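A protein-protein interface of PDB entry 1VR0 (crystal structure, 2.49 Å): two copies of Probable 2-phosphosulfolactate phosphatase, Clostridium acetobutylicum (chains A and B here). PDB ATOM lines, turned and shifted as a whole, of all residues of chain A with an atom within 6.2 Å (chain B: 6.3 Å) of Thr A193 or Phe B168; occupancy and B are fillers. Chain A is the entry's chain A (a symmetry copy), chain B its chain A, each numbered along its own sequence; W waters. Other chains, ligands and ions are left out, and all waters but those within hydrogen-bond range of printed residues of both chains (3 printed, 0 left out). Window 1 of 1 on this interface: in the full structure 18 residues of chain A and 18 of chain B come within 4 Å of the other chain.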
ATOM      1  N   PHE A 163      14.801 -28.445 -15.248  1.00  0.00           N
ATOM      2  CA  PHE A 163      14.235 -27.154 -15.483  1.00  0.00           C
ATOM      3  C   PHE A 163      13.521 -26.685 -14.222  1.00  0.00           C
ATOM      4  O   PHE A 163      12.652 -27.397 -13.698  1.00  0.00           O
ATOM      5  CB  PHE A 163      13.248 -27.327 -16.667  1.00  0.00           C
ATOM      6  CG  PHE A 163      12.646 -26.071 -17.155  1.00  0.00           C
ATOM      7  CD1 PHE A 163      11.769 -25.351 -16.369  1.00  0.00           C
ATOM      8  CD2 PHE A 163      12.896 -25.638 -18.428  1.00  0.00           C
ATOM      9  CE1 PHE A 163      11.166 -24.196 -16.835  1.00  0.00           C
ATOM     10  CE2 PHE A 163      12.296 -24.482 -18.915  1.00  0.00           C
ATOM     11  CZ  PHE A 163      11.424 -23.766 -18.104  1.00  0.00           C
ATOM     12  N   PHE A 168      14.582 -19.900 -14.344  1.00  0.00           N
ATOM     13  CA  PHE A 168      14.136 -19.549 -15.674  1.00  0.00           C
ATOM     14  C   PHE A 168      13.616 -18.117 -15.708  1.00  0.00           C
ATOM     15  O   PHE A 168      13.965 -17.349 -16.614  1.00  0.00           O
ATOM     16  CB  PHE A 168      13.045 -20.523 -16.099  1.00  0.00           C
ATOM     17  CG  PHE A 168      12.681 -20.484 -17.582  1.00  0.00           C
ATOM     18  CD1 PHE A 168      13.556 -20.969 -18.541  1.00  0.00           C
ATOM     19  CD2 PHE A 168      11.425 -20.046 -18.000  1.00  0.00           C
ATOM     20  CE1 PHE A 168      13.207 -20.964 -19.902  1.00  0.00           C
ATOM     21  CE2 PHE A 168      11.083 -20.049 -19.345  1.00  0.00           C
ATOM     22  CZ  PHE A 168      11.976 -20.519 -20.296  1.00  0.00           C
ATOM     23  N   THR A 188      17.650 -17.088 -28.714  1.00  0.00           N
ATOM     24  CA  THR A 188      17.125 -18.405 -29.035  1.00  0.00           C
ATOM     25  C   THR A 188      15.719 -18.503 -28.469  1.00  0.00           C
ATOM     26  O   THR A 188      15.338 -17.710 -27.603  1.00  0.00           O
ATOM     27  CB  THR A 188      17.946 -19.558 -28.447  1.00  0.00           C
ATOM     28  OG1 THR A 188      17.899 -19.530 -27.012  1.00  0.00           O
ATOM     29  CG2 THR A 188      19.337 -19.501 -28.908  1.00  0.00           C
ATOM     30  N   ASP A 189      14.965 -19.483 -28.948  1.00  0.00           N
ATOM     31  CA  ASP A 189      13.588 -19.657 -28.504  1.00  0.00           C
ATOM     32  C   ASP A 189      13.514 -19.854 -26.969  1.00  0.00           C
ATOM     33  O   ASP A 189      12.582 -19.394 -26.326  1.00  0.00           O
ATOM     34  CB  ASP A 189      12.942 -20.833 -29.246  1.00  0.00           C
ATOM     35  CG  ASP A 189      12.444 -20.461 -30.636  1.00  0.00           C
ATOM     36  OD1 ASP A 189      12.890 -19.426 -31.196  1.00  0.00           O
ATOM     37  OD2 ASP A 189      11.585 -21.206 -31.190  1.00  0.00           O
ATOM     38  N   ALA A 190      14.506 -20.536 -26.394  1.00  0.00           N
ATOM     39  CA  ALA A 190      14.549 -20.765 -24.949  1.00  0.00           C
ATOM     40  C   ALA A 190      14.664 -19.466 -24.203  1.00  0.00           C
ATOM     41  O   ALA A 190      14.003 -19.279 -23.186  1.00  0.00           O
ATOM     42  CB  ALA A 190      15.711 -21.686 -24.564  1.00  0.00           C
ATOM     43  N   ALA A 191      15.495 -18.564 -24.725  1.00  0.00           N
ATOM     44  CA  ALA A 191      15.696 -17.232 -24.146  1.00  0.00           C
ATOM     45  C   ALA A 191      14.480 -16.338 -24.332  1.00  0.00           C
ATOM     46  O   ALA A 191      14.035 -15.712 -23.401  1.00  0.00           O
ATOM     47  CB  ALA A 191      16.895 -16.616 -24.749  1.00  0.00           C
ATOM     48  N   THR A 192      13.946 -16.304 -25.542  1.00  0.00           N
ATOM     49  CA  THR A 192      12.700 -15.615 -25.832  1.00  0.00           C
ATOM     50  C   THR A 192      11.591 -16.038 -24.846  1.00  0.00           C
ATOM     51  O   THR A 192      10.876 -15.210 -24.290  1.00  0.00           O
ATOM     52  CB  THR A 192      12.259 -15.938 -27.269  1.00  0.00           C
ATOM     53  OG1 THR A 192      13.205 -15.401 -28.200  1.00  0.00           O
ATOM     54  CG2 THR A 192      10.906 -15.410 -27.546  1.00  0.00           C
ATOM     55  N   THR A 193      11.470 -17.336 -24.608  1.00  0.00           N
ATOM     56  CA  THR A 193      10.427 -17.868 -23.718  1.00  0.00           C
ATOM     57  C   THR A 193      10.633 -17.444 -22.261  1.00  0.00           C
ATOM     58  O   THR A 193       9.691 -17.034 -21.593  1.00  0.00           O
ATOM     59  CB  THR A 193      10.329 -19.396 -23.841  1.00  0.00           C
ATOM     60  OG1 THR A 193      10.149 -19.764 -25.224  1.00  0.00           O
ATOM     61  CG2 THR A 193       9.124 -19.952 -23.038  1.00  0.00           C
ATOM     62  N   ALA A 194      11.868 -17.498 -21.771  1.00  0.00           N
ATOM     63  CA  ALA A 194      12.178 -16.997 -20.434  1.00  0.00           C
ATOM     64  C   ALA A 194      11.812 -15.525 -20.319  1.00  0.00           C
ATOM     65  O   ALA A 194      11.153 -15.123 -19.369  1.00  0.00           O
ATOM     66  CB  ALA A 194      13.629 -17.169 -20.130  1.00  0.00           C
ATOM     67  N   GLN A 195      12.247 -14.719 -21.281  1.00  0.00           N
ATOM     68  CA  GLN A 195      11.963 -13.304 -21.255  1.00  0.00           C
ATOM     69  C   GLN A 195      10.454 -13.051 -21.240  1.00  0.00           C
ATOM     70  O   GLN A 195       9.975 -12.158 -20.548  1.00  0.00           O
ATOM     71  CB  GLN A 195      12.647 -12.642 -22.457  1.00  0.00           C
ATOM     72  CG  GLN A 195      12.668 -11.124 -22.432  1.00  0.00           C
ATOM     73  CD  GLN A 195      11.425 -10.515 -22.981  1.00  0.00           C
ATOM     74  OE1 GLN A 195      10.739 -11.136 -23.818  1.00  0.00           O
ATOM     75  NE2 GLN A 195      11.062  -9.313 -22.486  1.00  0.00           N
ATOM     76  N   TYR A 196       9.716 -13.868 -21.981  1.00  0.00           N
ATOM     77  CA  TYR A 196       8.264 -13.773 -22.048  1.00  0.00           C
ATOM     78  C   TYR A 196       7.622 -14.023 -20.699  1.00  0.00           C
ATOM     79  O   TYR A 196       6.715 -13.265 -20.286  1.00  0.00           O
ATOM     80  CB  TYR A 196       7.688 -14.764 -23.065  1.00  0.00           C
ATOM     81  CG  TYR A 196       6.184 -14.836 -22.975  1.00  0.00           C
ATOM     82  CD1 TYR A 196       5.393 -13.793 -23.438  1.00  0.00           C
ATOM     83  CD2 TYR A 196       5.543 -15.943 -22.390  1.00  0.00           C
ATOM     84  CE1 TYR A 196       4.003 -13.844 -23.333  1.00  0.00           C
ATOM     85  CE2 TYR A 196       4.159 -16.003 -22.289  1.00  0.00           C
ATOM     86  CZ  TYR A 196       3.389 -14.947 -22.757  1.00  0.00           C
ATOM     87  OH  TYR A 196       2.008 -14.994 -22.641  1.00  0.00           O
ATOM     88  N   VAL A 197       8.096 -15.076 -20.020  1.00  0.00           N
ATOM     89  CA  VAL A 197       7.602 -15.443 -18.700  1.00  0.00           C
ATOM     90  C   VAL A 197       7.871 -14.304 -17.721  1.00  0.00           C
ATOM     91  O   VAL A 197       6.977 -13.931 -16.909  1.00  0.00           O
ATOM     92  CB  VAL A 197       8.271 -16.740 -18.185  1.00  0.00           C
ATOM     93  CG1 VAL A 197       7.912 -17.005 -16.718  1.00  0.00           C
ATOM     94  CG2 VAL A 197       7.863 -17.910 -19.034  1.00  0.00           C
ATOM     95  N   TYR A 198       9.087 -13.749 -17.789  1.00  0.00           N
ATOM     96  CA  TYR A 198       9.429 -12.610 -16.932  1.00  0.00           C
ATOM     97  C   TYR A 198       8.547 -11.404 -17.259  1.00  0.00           C
ATOM     98  O   TYR A 198       7.897 -10.846 -16.383  1.00  0.00           O
ATOM     99  CB  TYR A 198      10.902 -12.203 -17.040  1.00  0.00           C
ATOM    100  CG  TYR A 198      11.087 -10.861 -16.428  1.00  0.00           C
ATOM    101  CD1 TYR A 198      11.112 -10.731 -15.044  1.00  0.00           C
ATOM    102  CD2 TYR A 198      11.115  -9.689 -17.213  1.00  0.00           C
ATOM    103  CE1 TYR A 198      11.203  -9.483 -14.440  1.00  0.00           C
ATOM    104  CE2 TYR A 198      11.220  -8.427 -16.608  1.00  0.00           C
ATOM    105  CZ  TYR A 198      11.275  -8.337 -15.218  1.00  0.00           C
ATOM    106  OH  TYR A 198      11.380  -7.128 -14.554  1.00  0.00           O
ATOM    107  N   LEU B  17       8.458 -32.829 -19.678  1.00  0.00           N
ATOM    108  CA  LEU B  17       8.686 -32.329 -21.023  1.00  0.00           C
ATOM    109  C   LEU B  17      10.189 -32.344 -21.321  1.00  0.00           C
ATOM    110  O   LEU B  17      10.999 -31.980 -20.468  1.00  0.00           O
ATOM    111  CB  LEU B  17       8.135 -30.922 -21.139  1.00  0.00           C
ATOM    112  CG  LEU B  17       8.240 -30.295 -22.514  1.00  0.00           C
ATOM    113  CD1 LEU B  17       7.050 -29.358 -22.692  1.00  0.00           C
ATOM    114  CD2 LEU B  17       9.545 -29.532 -22.725  1.00  0.00           C
ATOM    115  N   ILE B  19      12.907 -30.876 -24.174  1.00  0.00           N
ATOM    116  CA  ILE B  19      12.881 -29.709 -25.026  1.00  0.00           C
ATOM    117  C   ILE B  19      13.421 -29.917 -26.460  1.00  0.00           C
ATOM    118  O   ILE B  19      13.244 -29.022 -27.287  1.00  0.00           O
ATOM    119  CB  ILE B  19      13.644 -28.541 -24.386  1.00  0.00           C
ATOM    120  CG1 ILE B  19      15.120 -28.919 -24.151  1.00  0.00           C
ATOM    121  CG2 ILE B  19      12.981 -28.138 -23.078  1.00  0.00           C
ATOM    122  CD1 ILE B  19      16.061 -27.693 -24.128  1.00  0.00           C
ATOM    123  N   ILE B  37       6.390 -34.649 -30.415  1.00  0.00           N
ATOM    124  CA  ILE B  37       5.851 -33.478 -31.106  1.00  0.00           C
ATOM    125  C   ILE B  37       6.860 -32.830 -32.054  1.00  0.00           C
ATOM    126  O   ILE B  37       7.954 -32.454 -31.658  1.00  0.00           O
ATOM    127  CB  ILE B  37       5.301 -32.473 -30.080  1.00  0.00           C
ATOM    128  CG1 ILE B  37       4.094 -33.109 -29.377  1.00  0.00           C
ATOM    129  CG2 ILE B  37       4.828 -31.207 -30.739  1.00  0.00           C
ATOM    130  CD1 ILE B  37       3.711 -32.409 -28.114  1.00  0.00           C
ATOM    131  N   ASN B 156       9.519 -32.939 -27.162  1.00  0.00           N
ATOM    132  CA  ASN B 156       9.610 -31.969 -28.252  1.00  0.00           C
ATOM    133  C   ASN B 156      10.755 -32.353 -29.178  1.00  0.00           C
ATOM    134  O   ASN B 156      11.840 -32.652 -28.712  1.00  0.00           O
ATOM    135  CB  ASN B 156       9.885 -30.566 -27.686  1.00  0.00           C
ATOM    136  CG  ASN B 156       8.731 -30.039 -26.858  1.00  0.00           C
ATOM    137  OD1 ASN B 156       7.984 -30.807 -26.275  1.00  0.00           O
ATOM    138  ND2 ASN B 156       8.558 -28.741 -26.840  1.00  0.00           N
ATOM    139  N   PHE B 163      15.440 -26.148 -28.269  1.00  0.00           N
ATOM    140  CA  PHE B 163      14.159 -25.703 -27.818  1.00  0.00           C
ATOM    141  C   PHE B 163      13.501 -24.882 -28.919  1.00  0.00           C
ATOM    142  O   PHE B 163      14.094 -23.911 -29.411  1.00  0.00           O
ATOM    143  CB  PHE B 163      14.422 -24.851 -26.550  1.00  0.00           C
ATOM    144  CG  PHE B 163      13.205 -24.397 -25.849  1.00  0.00           C
ATOM    145  CD1 PHE B 163      12.348 -23.486 -26.433  1.00  0.00           C
ATOM    146  CD2 PHE B 163      12.946 -24.822 -24.575  1.00  0.00           C
ATOM    147  CE1 PHE B 163      11.228 -23.022 -25.766  1.00  0.00           C
ATOM    148  CE2 PHE B 163      11.829 -24.362 -23.888  1.00  0.00           C
ATOM    149  CZ  PHE B 163      10.971 -23.453 -24.497  1.00  0.00           C
ATOM    150  N   SER B 164      12.265 -25.243 -29.267  1.00  0.00           N
ATOM    151  CA  SER B 164      11.497 -24.540 -30.287  1.00  0.00           C
ATOM    152  C   SER B 164      10.112 -24.205 -29.758  1.00  0.00           C
ATOM    153  O   SER B 164       9.386 -25.069 -29.249  1.00  0.00           O
ATOM    154  CB  SER B 164      11.381 -25.394 -31.534  1.00  0.00           C
ATOM    155  OG  SER B 164      11.217 -24.580 -32.677  1.00  0.00           O
ATOM    156  N   ILE B 165       9.754 -22.934 -29.885  1.00  0.00           N
ATOM    157  CA  ILE B 165       8.466 -22.424 -29.402  1.00  0.00           C
ATOM    158  C   ILE B 165       7.241 -23.145 -29.966  1.00  0.00           C
ATOM    159  O   ILE B 165       6.266 -23.334 -29.251  1.00  0.00           O
ATOM    160  CB  ILE B 165       8.369 -20.901 -29.630  1.00  0.00           C
ATOM    161  CG1 ILE B 165       9.055 -20.187 -28.459  1.00  0.00           C
ATOM    162  CG2 ILE B 165       6.932 -20.456 -29.761  1.00  0.00           C
ATOM    163  CD1 ILE B 165       9.260 -18.710 -28.624  1.00  0.00           C
ATOM    164  N   ASP B 166       7.282 -23.547 -31.234  1.00  0.00           N
ATOM    165  CA  ASP B 166       6.138 -24.293 -31.832  1.00  0.00           C
ATOM    166  C   ASP B 166       5.889 -25.598 -31.060  1.00  0.00           C
ATOM    167  O   ASP B 166       4.766 -25.870 -30.605  1.00  0.00           O
ATOM    168  CB  ASP B 166       6.342 -24.579 -33.344  1.00  0.00           C
ATOM    169  CG  ASP B 166       7.716 -25.167 -33.673  1.00  0.00           C
ATOM    170  OD1 ASP B 166       8.646 -25.123 -32.843  1.00  0.00           O
ATOM    171  OD2 ASP B 166       7.887 -25.672 -34.786  1.00  0.00           O
ATOM    172  N   ASP B 167       6.930 -26.403 -30.879  1.00  0.00           N
ATOM    173  CA  ASP B 167       6.731 -27.684 -30.224  1.00  0.00           C
ATOM    174  C   ASP B 167       6.341 -27.467 -28.753  1.00  0.00           C
ATOM    175  O   ASP B 167       5.588 -28.221 -28.197  1.00  0.00           O
ATOM    176  CB  ASP B 167       7.980 -28.590 -30.370  1.00  0.00           C
ATOM    177  CG  ASP B 167       8.220 -29.023 -31.830  1.00  0.00           C
ATOM    178  OD1 ASP B 167       7.237 -29.092 -32.569  1.00  0.00           O
ATOM    179  OD2 ASP B 167       9.360 -29.289 -32.251  1.00  0.00           O
ATOM    180  N   PHE B 168       6.850 -26.413 -28.144  1.00  0.00           N
ATOM    181  CA  PHE B 168       6.641 -26.149 -26.739  1.00  0.00           C
ATOM    182  C   PHE B 168       5.198 -25.736 -26.475  1.00  0.00           C
ATOM    183  O   PHE B 168       4.568 -26.239 -25.537  1.00  0.00           O
ATOM    184  CB  PHE B 168       7.599 -25.050 -26.298  1.00  0.00           C
ATOM    185  CG  PHE B 168       7.724 -24.864 -24.786  1.00  0.00           C
ATOM    186  CD1 PHE B 168       8.370 -25.808 -24.005  1.00  0.00           C
ATOM    187  CD2 PHE B 168       7.273 -23.697 -24.170  1.00  0.00           C
ATOM    188  CE1 PHE B 168       8.514 -25.620 -22.620  1.00  0.00           C
ATOM    189  CE2 PHE B 168       7.423 -23.514 -22.802  1.00  0.00           C
ATOM    190  CZ  PHE B 168       8.054 -24.476 -22.029  1.00  0.00           C
ATOM    191  N   ILE B 169       4.652 -24.835 -27.298  1.00  0.00           N
ATOM    192  CA  ILE B 169       3.287 -24.388 -27.067  1.00  0.00           C
ATOM    193  C   ILE B 169       2.311 -25.520 -27.353  1.00  0.00           C
ATOM    194  O   ILE B 169       1.271 -25.651 -26.704  1.00  0.00           O
ATOM    195  CB  ILE B 169       2.935 -23.113 -27.866  1.00  0.00           C
ATOM    196  CG1 ILE B 169       1.578 -22.548 -27.392  1.00  0.00           C
ATOM    197  CG2 ILE B 169       2.936 -23.346 -29.357  1.00  0.00           C
ATOM    198  CD1 ILE B 169       1.331 -21.065 -27.795  1.00  0.00           C
ATOM    199  N   CYS B 170       2.652 -26.339 -28.342  1.00  0.00           N
ATOM    200  CA  CYS B 170       1.838 -27.483 -28.694  1.00  0.00           C
ATOM    201  C   CYS B 170       1.831 -28.464 -27.534  1.00  0.00           C
ATOM    202  O   CYS B 170       0.790 -28.995 -27.217  1.00  0.00           O
ATOM    203  CB  CYS B 170       2.384 -28.149 -29.943  1.00  0.00           C
ATOM    204  SG  CYS B 170       1.327 -29.512 -30.496  1.00  0.00           S
ATOM    205  N   SER B 171       2.984 -28.657 -26.879  1.00  0.00           N
ATOM    206  CA  SER B 171       3.029 -29.447 -25.638  1.00  0.00           C
ATOM    207  C   SER B 171       2.075 -28.906 -24.600  1.00  0.00           C
ATOM    208  O   SER B 171       1.355 -29.644 -23.962  1.00  0.00           O
ATOM    209  CB  SER B 171       4.397 -29.435 -25.010  1.00  0.00           C
ATOM    210  OG  SER B 171       5.393 -29.892 -25.903  1.00  0.00           O
ATOM    211  N   GLY B 172       2.095 -27.596 -24.428  1.00  0.00           N
ATOM    212  CA  GLY B 172       1.221 -26.907 -23.497  1.00  0.00           C
ATOM    213  C   GLY B 172      -0.241 -27.118 -23.778  1.00  0.00           C
ATOM    214  O   GLY B 172      -1.017 -27.310 -22.857  1.00  0.00           O
ATOM    215  N   TYR B 173      -0.613 -27.063 -25.048  1.00  0.00           N
ATOM    216  CA  TYR B 173      -1.986 -27.293 -25.440  1.00  0.00           C
ATOM    217  C   TYR B 173      -2.434 -28.675 -25.027  1.00  0.00           C
ATOM    218  O   TYR B 173      -3.554 -28.850 -24.500  1.00  0.00           O
ATOM    219  CB  TYR B 173      -2.113 -27.135 -26.954  1.00  0.00           C
ATOM    220  CG  TYR B 173      -3.383 -27.639 -27.545  1.00  0.00           C
ATOM    221  CD1 TYR B 173      -4.618 -27.219 -27.065  1.00  0.00           C
ATOM    222  CD2 TYR B 173      -3.356 -28.500 -28.643  1.00  0.00           C
ATOM    223  CE1 TYR B 173      -5.788 -27.660 -27.662  1.00  0.00           C
ATOM    224  CE2 TYR B 173      -4.514 -28.937 -29.233  1.00  0.00           C
ATOM    225  CZ  TYR B 173      -5.724 -28.526 -28.744  1.00  0.00           C
ATOM    226  OH  TYR B 173      -6.882 -28.998 -29.354  1.00  0.00           O
ATOM    227  N   ASP B 189       8.254 -28.510 -13.749  1.00  0.00           N
ATOM    228  CA  ASP B 189       8.297 -27.082 -14.037  1.00  0.00           C
ATOM    229  C   ASP B 189       8.299 -26.818 -15.564  1.00  0.00           C
ATOM    230  O   ASP B 189       7.713 -25.852 -16.030  1.00  0.00           O
ATOM    231  CB  ASP B 189       9.519 -26.447 -13.363  1.00  0.00           C
ATOM    232  CG  ASP B 189       9.293 -26.140 -11.888  1.00  0.00           C
ATOM    233  OD1 ASP B 189       8.361 -26.717 -11.271  1.00  0.00           O
ATOM    234  OD2 ASP B 189      10.054 -25.302 -11.323  1.00  0.00           O
ATOM    235  N   ALA B 190       8.958 -27.688 -16.331  1.00  0.00           N
ATOM    236  CA  ALA B 190       9.010 -27.547 -17.788  1.00  0.00           C
ATOM    237  C   ALA B 190       7.637 -27.664 -18.387  1.00  0.00           C
ATOM    238  O   ALA B 190       7.290 -26.904 -19.287  1.00  0.00           O
ATOM    239  CB  ALA B 190       9.938 -28.591 -18.417  1.00  0.00           C
ATOM    240  N   ALA B 191       6.852 -28.610 -17.871  1.00  0.00           N
ATOM    241  CA  ALA B 191       5.473 -28.833 -18.312  1.00  0.00           C
ATOM    242  C   ALA B 191       4.543 -27.711 -17.876  1.00  0.00           C
ATOM    243  O   ALA B 191       3.784 -27.205 -18.666  1.00  0.00           O
ATOM    244  CB  ALA B 191       5.001 -30.133 -17.794  1.00  0.00           C
ATOM    245  N   THR B 193       5.403 -24.692 -17.348  1.00  0.00           N
ATOM    246  CA  THR B 193       5.763 -23.520 -18.159  1.00  0.00           C
ATOM    247  C   THR B 193       5.176 -23.584 -19.572  1.00  0.00           C
ATOM    248  O   THR B 193       4.636 -22.601 -20.067  1.00  0.00           O
ATOM    249  CB  THR B 193       7.288 -23.331 -18.202  1.00  0.00           C
ATOM    250  OG1 THR B 193       7.813 -23.288 -16.860  1.00  0.00           O
ATOM    251  CG2 THR B 193       7.675 -22.006 -18.910  1.00  0.00           C
ATOM    252  N   ALA B 194       5.236 -24.748 -20.212  1.00  0.00           N
ATOM    253  CA  ALA B 194       4.592 -24.935 -21.511  1.00  0.00           C
ATOM    254  C   ALA B 194       3.099 -24.660 -21.408  1.00  0.00           C
ATOM    255  O   ALA B 194       2.548 -23.923 -22.218  1.00  0.00           O
ATOM    256  CB  ALA B 194       4.804 -26.325 -22.009  1.00  0.00           C
ATOM    257  N   GLN B 195       2.443 -25.256 -20.420  1.00  0.00           N
ATOM    258  CA  GLN B 195       1.022 -25.069 -20.248  1.00  0.00           C
ATOM    259  C   GLN B 195       0.687 -23.589 -20.048  1.00  0.00           C
ATOM    260  O   GLN B 195      -0.308 -23.096 -20.568  1.00  0.00           O
ATOM    261  CB  GLN B 195       0.551 -25.932 -19.071  1.00  0.00           C
ATOM    262  CG  GLN B 195      -0.955 -26.053 -18.922  1.00  0.00           C
ATOM    263  CD  GLN B 195      -1.559 -24.927 -18.158  1.00  0.00           C
ATOM    264  OE1 GLN B 195      -0.878 -24.302 -17.320  1.00  0.00           O
ATOM    265  NE2 GLN B 195      -2.830 -24.593 -18.462  1.00  0.00           N
ATOM    266  N   VAL B 197       2.416 -20.973 -21.194  1.00  0.00           N
ATOM    267  CA  VAL B 197       2.590 -20.306 -22.477  1.00  0.00           C
ATOM    268  C   VAL B 197       1.356 -20.537 -23.344  1.00  0.00           C
ATOM    269  O   VAL B 197       0.838 -19.583 -23.991  1.00  0.00           O
ATOM    270  CB  VAL B 197       3.849 -20.820 -23.217  1.00  0.00           C
ATOM    271  CG1 VAL B 197       3.911 -20.277 -24.649  1.00  0.00           C
ATOM    272  CG2 VAL B 197       5.090 -20.434 -22.465  1.00  0.00           C
ATOM    273  N   TYR B 198       0.880 -21.788 -23.362  1.00  0.00           N
ATOM    274  CA  TYR B 198      -0.335 -22.106 -24.117  1.00  0.00           C
ATOM    275  C   TYR B 198      -1.537 -21.353 -23.546  1.00  0.00           C
ATOM    276  O   TYR B 198      -2.233 -20.645 -24.265  1.00  0.00           O
ATOM    277  CB  TYR B 198      -0.645 -23.606 -24.145  1.00  0.00           C
ATOM    278  CG  TYR B 198      -2.040 -23.811 -24.615  1.00  0.00           C
ATOM    279  CD1 TYR B 198      -2.338 -23.684 -25.968  1.00  0.00           C
ATOM    280  CD2 TYR B 198      -3.104 -24.010 -23.710  1.00  0.00           C
ATOM    281  CE1 TYR B 198      -3.644 -23.790 -26.430  1.00  0.00           C
ATOM    282  CE2 TYR B 198      -4.423 -24.131 -24.173  1.00  0.00           C
ATOM    283  CZ  TYR B 198      -4.680 -24.030 -25.540  1.00  0.00           C
ATOM    284  OH  TYR B 198      -5.954 -24.140 -26.067  1.00  0.00           O
ATOM    285  N   PHE B 207       1.596 -16.848 -31.162  1.00  0.00           N
ATOM    286  CA  PHE B 207       2.808 -16.948 -30.401  1.00  0.00           C
ATOM    287  C   PHE B 207       3.881 -17.730 -31.148  1.00  0.00           C
ATOM    288  O   PHE B 207       5.067 -17.516 -30.968  1.00  0.00           O
ATOM    289  CB  PHE B 207       2.477 -17.579 -29.047  1.00  0.00           C
ATOM    290  CG  PHE B 207       3.570 -17.481 -28.079  1.00  0.00           C
ATOM    291  CD1 PHE B 207       3.680 -16.376 -27.269  1.00  0.00           C
ATOM    292  CD2 PHE B 207       4.536 -18.477 -28.007  1.00  0.00           C
ATOM    293  CE1 PHE B 207       4.745 -16.269 -26.379  1.00  0.00           C
ATOM    294  CE2 PHE B 207       5.611 -18.377 -27.107  1.00  0.00           C
ATOM    295  CZ  PHE B 207       5.702 -17.292 -26.296  1.00  0.00           C
HETATM  296  O   HOH W   1      15.928 -22.350 -28.268  1.00  0.00           O
HETATM  297  O   HOH W   2      11.063 -29.189 -14.869  1.00  0.00           O
HETATM  298  O   HOH W   3      12.176 -22.131 -33.580  1.00  0.00           O
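Among the printed residues, merely in contact across the chains: Phe A163 with Asp B189 (3.3 Å), Phe A163 with Ala B190 (3.7 Å), Phe A163 with Thr B193 (3.5 Å), Phe A168 with Thr B193 (3.95 Å), Asp A189 with Phe B163 (3.3 Å), Asp A189 with Ser B164 (3.5 Å), Ala A190 with Phe B163 (3.7 Å), Thr A192 with Ile B165 (3.8 Å), Thr A193 with Phe B163 (3.5 Å), Thr A193 with Ile B165 (3.4 Å), Thr A193 with Phe B168 (3.95 Å) and Tyr A196 with Phe B207 (3.9 Å).
Hydrophobic or aromatic side chains of chain B that line the printed part of chain A: Phe B163, Ile B165, Phe B168, Ala B190 and Phe B207.
Among the printed residues, 13 pairs touch across the chains.
Among the printed residues, no Asp or Glu carboxylate lies within 4 Å of a Lys or Arg side-chain nitrogen of the other chain.
OD2 of Asp A189 is in hydrogen-bond range of N of Ile B165.
Printed residues of chain B within 4 Å of Asp A189: Phe B163 (3.3 Å), Ser B164 (3.5 Å) and Ile B165 (2.8 Å).
Of the printed residues of chain B, Thr A192 touches Ile B165 (3.8 Å).
Of the printed residues of chain B, Thr A193 touches Phe B163 (3.5 Å), Ile B165 (3.4 Å) and Phe B168 (3.95 Å).
Of the printed residues of chain A, Ser B164 touches Asp A189.
Phe B168 touches just one residue of chain A: Thr A193.
Printed residues of chain A within 4 Å of Thr B193: Phe A163 (3.5 Å) and Phe A168 (3.95 Å).
Tyr B198 touches none of the printed residues of chain A.
The nearest printed residue of chain B that does not touch Thr A192 is Phe B207 (5.7 Å).
ND2 of Asn B156 lies close to N of Phe B168, 3.2 Å away.
OG of Ser B164 is in hydrogen-bond range of OD1 of Asp B166 (2.6 Å).
The side-chain hydroxyl of Thr B193 is in hydrogen-bond range of the backbone carbonyl oxygen of Asp B189 (2.7 Å).
The backbone carbonyl oxygen of Thr A188 is in hydrogen-bond range of the side-chain hydroxyl of Thr A192 (3.2 Å).
The backbone carbonyl oxygen (O) of Asp A189 lies within hydrogen-bond range of the side-chain hydroxyl (OG1) of Thr A193 (2.7 Å).
Water W3 lies within hydrogen-bond range of OD2 of Asp A189 (2.6 Å) and OG of Ser B164 (2.8 Å).
Water W2 lies within hydrogen-bond range of O of Phe A163 (2.7 Å), N of Ala B190 (3.0 Å) and N of Asp B189 (3.1 Å).
Water W1 lies within hydrogen-bond range of the backbone carbonyl oxygen (O) of Phe B163, the backbone NH (N) of Ala A190 and the backbone NH (N) of Asp A189.
Phe A163 touches Asp B189, and with the chains exchanged Asp A189 touches Phe B163.
Phe A163 touches Ala B190, and with the chains exchanged Ala A190 touches Phe B163.
Phe A163 touches Thr B193, and with the chains exchanged Thr A193 touches Phe B163.
Phe A168 touches Thr B193, and with the chains exchanged Thr A193 touches Phe B168.
Positions printed for both chains: 163, 168, 189, 190, 191, 193, 194, 195, 197 and 198.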
